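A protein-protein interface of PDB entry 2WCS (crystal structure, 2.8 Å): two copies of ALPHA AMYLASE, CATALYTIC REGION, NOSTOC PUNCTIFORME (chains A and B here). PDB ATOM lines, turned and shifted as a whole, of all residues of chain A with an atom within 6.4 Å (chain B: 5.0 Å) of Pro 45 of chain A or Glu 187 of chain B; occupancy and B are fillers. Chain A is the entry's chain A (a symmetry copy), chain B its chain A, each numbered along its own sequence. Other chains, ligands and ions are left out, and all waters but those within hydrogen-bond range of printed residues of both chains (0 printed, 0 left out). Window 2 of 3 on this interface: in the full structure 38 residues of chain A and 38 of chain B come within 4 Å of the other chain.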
ATOM      1  N   LEU A  33      21.271   0.286   3.050  1.00  0.00           N
ATOM      2  CA  LEU A  33      22.670  -0.121   3.007  1.00  0.00           C
ATOM      3  C   LEU A  33      23.006  -1.064   4.158  1.00  0.00           C
ATOM      4  O   LEU A  33      23.639  -0.664   5.134  1.00  0.00           O
ATOM      5  CB  LEU A  33      23.586   1.103   3.045  1.00  0.00           C
ATOM      6  CG  LEU A  33      23.468   2.075   1.867  1.00  0.00           C
ATOM      7  CD1 LEU A  33      23.380   1.317   0.552  1.00  0.00           C
ATOM      8  CD2 LEU A  33      22.267   2.992   2.045  1.00  0.00           C
ATOM      9  N   TRP A  41      27.029   6.380   9.239  1.00  0.00           N
ATOM     10  CA  TRP A  41      25.574   6.416   9.333  1.00  0.00           C
ATOM     11  C   TRP A  41      25.017   7.835   9.409  1.00  0.00           C
ATOM     12  O   TRP A  41      23.998   8.142   8.789  1.00  0.00           O
ATOM     13  CB  TRP A  41      25.108   5.595  10.541  1.00  0.00           C
ATOM     14  CG  TRP A  41      23.619   5.433  10.621  1.00  0.00           C
ATOM     15  CD1 TRP A  41      22.756   6.135  11.413  1.00  0.00           C
ATOM     16  CD2 TRP A  41      22.813   4.525   9.858  1.00  0.00           C
ATOM     17  NE1 TRP A  41      21.463   5.722  11.192  1.00  0.00           N
ATOM     18  CE2 TRP A  41      21.469   4.735  10.243  1.00  0.00           C
ATOM     19  CE3 TRP A  41      23.097   3.555   8.887  1.00  0.00           C
ATOM     20  CZ2 TRP A  41      20.408   4.010   9.689  1.00  0.00           C
ATOM     21  CZ3 TRP A  41      22.040   2.834   8.335  1.00  0.00           C
ATOM     22  CH2 TRP A  41      20.713   3.068   8.740  1.00  0.00           C
ATOM     23  N   ASP A  42      25.685   8.700  10.168  1.00  0.00           N
ATOM     24  CA  ASP A  42      25.245  10.086  10.302  1.00  0.00           C
ATOM     25  C   ASP A  42      25.430  10.798   8.970  1.00  0.00           C
ATOM     26  O   ASP A  42      24.894  11.886   8.754  1.00  0.00           O
ATOM     27  CB  ASP A  42      26.060  10.802  11.380  1.00  0.00           C
ATOM     28  CG  ASP A  42      25.905  10.168  12.743  1.00  0.00           C
ATOM     29  OD1 ASP A  42      26.557  10.645  13.695  1.00  0.00           O
ATOM     30  OD2 ASP A  42      25.134   9.194  12.868  1.00  0.00           O
ATOM     31  N   SER A  43      26.197  10.168   8.084  1.00  0.00           N
ATOM     32  CA  SER A  43      26.484  10.712   6.760  1.00  0.00           C
ATOM     33  C   SER A  43      25.336  10.409   5.806  1.00  0.00           C
ATOM     34  O   SER A  43      25.152  11.095   4.797  1.00  0.00           O
ATOM     35  CB  SER A  43      27.768  10.090   6.205  1.00  0.00           C
ATOM     36  OG  SER A  43      28.788  10.052   7.189  1.00  0.00           O
ATOM     37  N   MET A  44      24.573   9.373   6.135  1.00  0.00           N
ATOM     38  CA  MET A  44      23.443   8.943   5.317  1.00  0.00           C
ATOM     39  C   MET A  44      22.121   9.326   5.972  1.00  0.00           C
ATOM     40  O   MET A  44      21.510   8.524   6.681  1.00  0.00           O
ATOM     41  CB  MET A  44      23.520   7.432   5.112  1.00  0.00           C
ATOM     42  CG  MET A  44      24.861   6.985   4.558  1.00  0.00           C
ATOM     43  SD  MET A  44      25.087   5.210   4.578  1.00  0.00           S
ATOM     44  CE  MET A  44      25.705   4.969   6.225  1.00  0.00           C
ATOM     45  N   PRO A  45      21.659  10.564   5.731  1.00  0.00           N
ATOM     46  CA  PRO A  45      20.414  11.124   6.267  1.00  0.00           C
ATOM     47  C   PRO A  45      19.202  10.213   6.102  1.00  0.00           C
ATOM     48  O   PRO A  45      18.616   9.750   7.081  1.00  0.00           O
ATOM     49  CB  PRO A  45      20.261  12.422   5.483  1.00  0.00           C
ATOM     50  CG  PRO A  45      21.672  12.837   5.254  1.00  0.00           C
ATOM     51  CD  PRO A  45      22.313  11.539   4.837  1.00  0.00           C
ATOM     52  N   THR A  46      18.835   9.972   4.849  1.00  0.00           N
ATOM     53  CA  THR A  46      17.690   9.137   4.505  1.00  0.00           C
ATOM     54  C   THR A  46      17.537   7.905   5.395  1.00  0.00           C
ATOM     55  O   THR A  46      16.463   7.668   5.951  1.00  0.00           O
ATOM     56  CB  THR A  46      17.774   8.693   3.034  1.00  0.00           C
ATOM     57  OG1 THR A  46      17.974   9.844   2.201  1.00  0.00           O
ATOM     58  CG2 THR A  46      16.493   8.000   2.612  1.00  0.00           C
ATOM     59  N   LEU A  47      18.604   7.128   5.535  1.00  0.00           N
ATOM     60  CA  LEU A  47      18.553   5.927   6.363  1.00  0.00           C
ATOM     61  C   LEU A  47      18.663   6.227   7.852  1.00  0.00           C
ATOM     62  O   LEU A  47      18.087   5.524   8.682  1.00  0.00           O
ATOM     63  CB  LEU A  47      19.661   4.954   5.962  1.00  0.00           C
ATOM     64  CG  LEU A  47      19.568   4.385   4.547  1.00  0.00           C
ATOM     65  CD1 LEU A  47      20.281   5.310   3.565  1.00  0.00           C
ATOM     66  CD2 LEU A  47      20.192   3.003   4.528  1.00  0.00           C
ATOM     67  N   GLN A  48      19.406   7.278   8.185  1.00  0.00           N
ATOM     68  CA  GLN A  48      19.662   7.624   9.578  1.00  0.00           C
ATOM     69  C   GLN A  48      18.383   8.075  10.276  1.00  0.00           C
ATOM     70  O   GLN A  48      18.121   7.695  11.418  1.00  0.00           O
ATOM     71  CB  GLN A  48      20.725   8.722   9.671  1.00  0.00           C
ATOM     72  CG  GLN A  48      21.079   9.123  11.094  1.00  0.00           C
ATOM     73  CD  GLN A  48      20.064  10.070  11.702  1.00  0.00           C
ATOM     74  OE1 GLN A  48      20.025  10.259  12.918  1.00  0.00           O
ATOM     75  NE2 GLN A  48      19.234  10.670  10.857  1.00  0.00           N
ATOM     76  N   GLY A  49      17.591   8.886   9.584  1.00  0.00           N
ATOM     77  CA  GLY A  49      16.321   9.348  10.115  1.00  0.00           C
ATOM     78  C   GLY A  49      15.157   9.021   9.201  1.00  0.00           C
ATOM     79  O   GLY A  49      14.441   9.913   8.749  1.00  0.00           O
ATOM     80  N   TYR A  50      14.968   7.734   8.929  1.00  0.00           N
ATOM     81  CA  TYR A  50      13.782   7.266   8.224  1.00  0.00           C
ATOM     82  C   TYR A  50      12.538   7.383   9.100  1.00  0.00           C
ATOM     83  O   TYR A  50      12.616   7.277  10.323  1.00  0.00           O
ATOM     84  CB  TYR A  50      13.966   5.817   7.766  1.00  0.00           C
ATOM     85  CG  TYR A  50      12.734   5.211   7.136  1.00  0.00           C
ATOM     86  CD1 TYR A  50      12.181   5.754   5.983  1.00  0.00           C
ATOM     87  CD2 TYR A  50      12.121   4.097   7.694  1.00  0.00           C
ATOM     88  CE1 TYR A  50      11.054   5.203   5.403  1.00  0.00           C
ATOM     89  CE2 TYR A  50      10.992   3.539   7.121  1.00  0.00           C
ATOM     90  CZ  TYR A  50      10.464   4.096   5.975  1.00  0.00           C
ATOM     91  OH  TYR A  50       9.342   3.545   5.402  1.00  0.00           O
ATOM     92  N   TRP B 147      15.001  10.229  -2.905  1.00  0.00           N
ATOM     93  CA  TRP B 147      16.340  10.093  -3.455  1.00  0.00           C
ATOM     94  C   TRP B 147      16.701  11.070  -4.558  1.00  0.00           C
ATOM     95  O   TRP B 147      17.583  10.796  -5.371  1.00  0.00           O
ATOM     96  CB  TRP B 147      16.540   8.665  -3.949  1.00  0.00           C
ATOM     97  CG  TRP B 147      16.391   7.671  -2.856  1.00  0.00           C
ATOM     98  CD1 TRP B 147      17.276   7.411  -1.845  1.00  0.00           C
ATOM     99  CD2 TRP B 147      15.263   6.834  -2.627  1.00  0.00           C
ATOM    100  NE1 TRP B 147      16.762   6.458  -0.999  1.00  0.00           N
ATOM    101  CE2 TRP B 147      15.526   6.087  -1.457  1.00  0.00           C
ATOM    102  CE3 TRP B 147      14.050   6.641  -3.297  1.00  0.00           C
ATOM    103  CZ2 TRP B 147      14.621   5.163  -0.942  1.00  0.00           C
ATOM    104  CZ3 TRP B 147      13.148   5.722  -2.783  1.00  0.00           C
ATOM    105  CH2 TRP B 147      13.437   4.994  -1.617  1.00  0.00           C
ATOM    106  N   TRP B 150      20.268  11.761  -5.175  1.00  0.00           N
ATOM    107  CA  TRP B 150      21.016  10.530  -5.435  1.00  0.00           C
ATOM    108  C   TRP B 150      21.473  10.630  -6.864  1.00  0.00           C
ATOM    109  O   TRP B 150      22.294   9.851  -7.329  1.00  0.00           O
ATOM    110  CB  TRP B 150      20.118   9.299  -5.298  1.00  0.00           C
ATOM    111  CG  TRP B 150      20.384   8.478  -4.081  1.00  0.00           C
ATOM    112  CD1 TRP B 150      20.477   8.925  -2.797  1.00  0.00           C
ATOM    113  CD2 TRP B 150      20.556   7.058  -4.027  1.00  0.00           C
ATOM    114  NE1 TRP B 150      20.694   7.872  -1.941  1.00  0.00           N
ATOM    115  CE2 TRP B 150      20.747   6.712  -2.668  1.00  0.00           C
ATOM    116  CE3 TRP B 150      20.567   6.044  -4.990  1.00  0.00           C
ATOM    117  CZ2 TRP B 150      20.945   5.388  -2.249  1.00  0.00           C
ATOM    118  CZ3 TRP B 150      20.764   4.725  -4.573  1.00  0.00           C
ATOM    119  CH2 TRP B 150      20.950   4.412  -3.213  1.00  0.00           C
ATOM    120  N   ASN B 185      27.534  11.841  -2.987  1.00  0.00           N
ATOM    121  CA  ASN B 185      26.582  11.351  -1.984  1.00  0.00           C
ATOM    122  C   ASN B 185      27.039  10.006  -1.424  1.00  0.00           C
ATOM    123  O   ASN B 185      26.985   8.986  -2.111  1.00  0.00           O
ATOM    124  CB  ASN B 185      25.200  11.190  -2.622  1.00  0.00           C
ATOM    125  CG  ASN B 185      24.104  10.948  -1.601  1.00  0.00           C
ATOM    126  OD1 ASN B 185      24.236  10.116  -0.701  1.00  0.00           O
ATOM    127  ND2 ASN B 185      23.006  11.672  -1.745  1.00  0.00           N
ATOM    128  N   PRO B 186      27.477   9.990  -0.155  1.00  0.00           N
ATOM    129  CA  PRO B 186      27.957   8.787   0.536  1.00  0.00           C
ATOM    130  C   PRO B 186      27.030   7.580   0.484  1.00  0.00           C
ATOM    131  O   PRO B 186      27.498   6.444   0.454  1.00  0.00           O
ATOM    132  CB  PRO B 186      28.201   9.280   1.963  1.00  0.00           C
ATOM    133  CG  PRO B 186      27.237  10.412   2.105  1.00  0.00           C
ATOM    134  CD  PRO B 186      27.371  11.118   0.784  1.00  0.00           C
ATOM    135  N   GLU B 187      25.723   7.826   0.480  1.00  0.00           N
ATOM    136  CA  GLU B 187      24.741   6.745   0.426  1.00  0.00           C
ATOM    137  C   GLU B 187      24.923   5.986  -0.878  1.00  0.00           C
ATOM    138  O   GLU B 187      24.827   4.763  -0.926  1.00  0.00           O
ATOM    139  CB  GLU B 187      23.318   7.298   0.476  1.00  0.00           C
ATOM    140  CG  GLU B 187      23.042   8.214   1.643  1.00  0.00           C
ATOM    141  CD  GLU B 187      21.564   8.432   1.862  1.00  0.00           C
ATOM    142  OE1 GLU B 187      20.835   8.605   0.864  1.00  0.00           O
ATOM    143  OE2 GLU B 187      21.136   8.437   3.031  1.00  0.00           O
ATOM    144  N   VAL B 188      25.174   6.739  -1.936  1.00  0.00           N
ATOM    145  CA  VAL B 188      25.388   6.174  -3.254  1.00  0.00           C
ATOM    146  C   VAL B 188      26.672   5.353  -3.235  1.00  0.00           C
ATOM    147  O   VAL B 188      26.731   4.238  -3.765  1.00  0.00           O
ATOM    148  CB  VAL B 188      25.495   7.296  -4.289  1.00  0.00           C
ATOM    149  CG1 VAL B 188      25.934   6.739  -5.617  1.00  0.00           C
ATOM    150  CG2 VAL B 188      24.146   8.008  -4.403  1.00  0.00           C
ATOM    151  N   ARG B 189      27.693   5.921  -2.602  1.00  0.00           N
ATOM    152  CA  ARG B 189      28.990   5.282  -2.466  1.00  0.00           C
ATOM    153  C   ARG B 189      28.756   3.912  -1.825  1.00  0.00           C
ATOM    154  O   ARG B 189      29.291   2.891  -2.267  1.00  0.00           O
ATOM    155  CB  ARG B 189      29.883   6.133  -1.555  1.00  0.00           C
ATOM    156  CG  ARG B 189      31.373   5.980  -1.779  1.00  0.00           C
ATOM    157  CD  ARG B 189      31.914   7.172  -2.551  1.00  0.00           C
ATOM    158  NE  ARG B 189      32.678   8.095  -1.711  1.00  0.00           N
ATOM    159  CZ  ARG B 189      33.864   7.816  -1.173  1.00  0.00           C
ATOM    160  NH1 ARG B 189      34.431   6.637  -1.380  1.00  0.00           N
ATOM    161  NH2 ARG B 189      34.494   8.722  -0.439  1.00  0.00           N
ATOM    162  N   GLU B 190      27.931   3.902  -0.787  1.00  0.00           N
ATOM    163  CA  GLU B 190      27.622   2.678  -0.064  1.00  0.00           C
ATOM    164  C   GLU B 190      26.911   1.620  -0.889  1.00  0.00           C
ATOM    165  O   GLU B 190      27.309   0.455  -0.893  1.00  0.00           O
ATOM    166  CB  GLU B 190      26.780   2.994   1.168  1.00  0.00           C
ATOM    167  CG  GLU B 190      27.526   2.770   2.442  1.00  0.00           C
ATOM    168  CD  GLU B 190      28.279   1.466   2.414  1.00  0.00           C
ATOM    169  OE1 GLU B 190      27.623   0.406   2.337  1.00  0.00           O
ATOM    170  OE2 GLU B 190      29.527   1.507   2.459  1.00  0.00           O
ATOM    171  N   TYR B 191      25.849   2.034  -1.571  1.00  0.00           N
ATOM    172  CA  TYR B 191      25.067   1.130  -2.394  1.00  0.00           C
ATOM    173  C   TYR B 191      25.951   0.457  -3.427  1.00  0.00           C
ATOM    174  O   TYR B 191      25.846  -0.752  -3.657  1.00  0.00           O
ATOM    175  CB  TYR B 191      23.948   1.903  -3.089  1.00  0.00           C
ATOM    176  CG  TYR B 191      23.027   1.041  -3.914  1.00  0.00           C
ATOM    177  CD1 TYR B 191      23.090   1.053  -5.305  1.00  0.00           C
ATOM    178  CD2 TYR B 191      22.078   0.222  -3.304  1.00  0.00           C
ATOM    179  CE1 TYR B 191      22.223   0.275  -6.070  1.00  0.00           C
ATOM    180  CE2 TYR B 191      21.210  -0.560  -4.060  1.00  0.00           C
ATOM    181  CZ  TYR B 191      21.286  -0.529  -5.439  1.00  0.00           C
ATOM    182  OH  TYR B 191      20.424  -1.296  -6.186  1.00  0.00           O
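The side-chain carboxylate (OE1) of Glu 187 of chain B sits at hydrogen-bond distance from the indole nitrogen (NE1) of Trp 150 of chain B (2.9 Å). The side-chain amide oxygen of Asn 185 of chain B sits at hydrogen-bond distance from the backbone NH of Glu 187 of chain B.
The backbone NH (N) of Thr 46 of chain A is in hydrogen-bond range of the side-chain carboxylate (OE2) of Glu 187 of chain B (3.3 Å). The backbone nitrogen (N) of Pro 45 of chain A lies close to the side-chain carboxylate (OE2) of Glu 187 of chain B (3.5 Å).
Of the 9 printed residues of chain B, 5 touch a printed residue of chain A. Of the 11 printed residues of chain A, 6 touch a printed residue of chain B. Printed residues of chain A that touch a printed residue of chain B: Leu 33, Ser 43, Met 44, Pro 45, Thr 46 and Leu 47. Among the printed residues, 8 pairs touch across the chains. Among the printed residues, no Asp or Glu carboxylate lies within 4 Å of a Lys or Arg side-chain nitrogen of the other chain.
No position is printed for both chains.
Among the printed residues, pairs that only touch across the chains: Leu 33 of chain A with Glu 190 of chain B (3.5 Å), Leu 33 of chain A with Tyr 191 of chain B (3.3 Å), Ser 43 of chain A with Pro 186 of chain B (3.5 Å), Met 44 of chain A with Glu 187 of chain B (3.2 Å), Thr 46 of chain A with Trp 147 of chain B (3.9 Å) and Leu 47 of chain A with Glu 187 of chain B (3.3 Å).
Of the printed residues of chain B, Leu 33 of chain A touches Glu 190 and Tyr 191. Printed residues of chain B within 4 Å of Ser 43 of chain A: Pro 186. Of chain B, only Glu 187 comes within 4 Å of Pro 45 of chain A. Of the printed residues of chain B, Thr 46 of chain A touches Trp 147 (3.9 Å) and Glu 187 (3.3 Å). Printed residues of chain B within 4 Å of Leu 47 of chain A: Glu 187. Of the printed residues of chain A, Glu 187 of chain B touches Met 44 (3.2 Å), Pro 45 (3.5 Å), Thr 46 (3.3 Å) and Leu 47 (3.3 Å). The nearest printed residue of chain A that does not touch Trp 147 of chain B is Leu 47 of chain A (5.9 Å).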
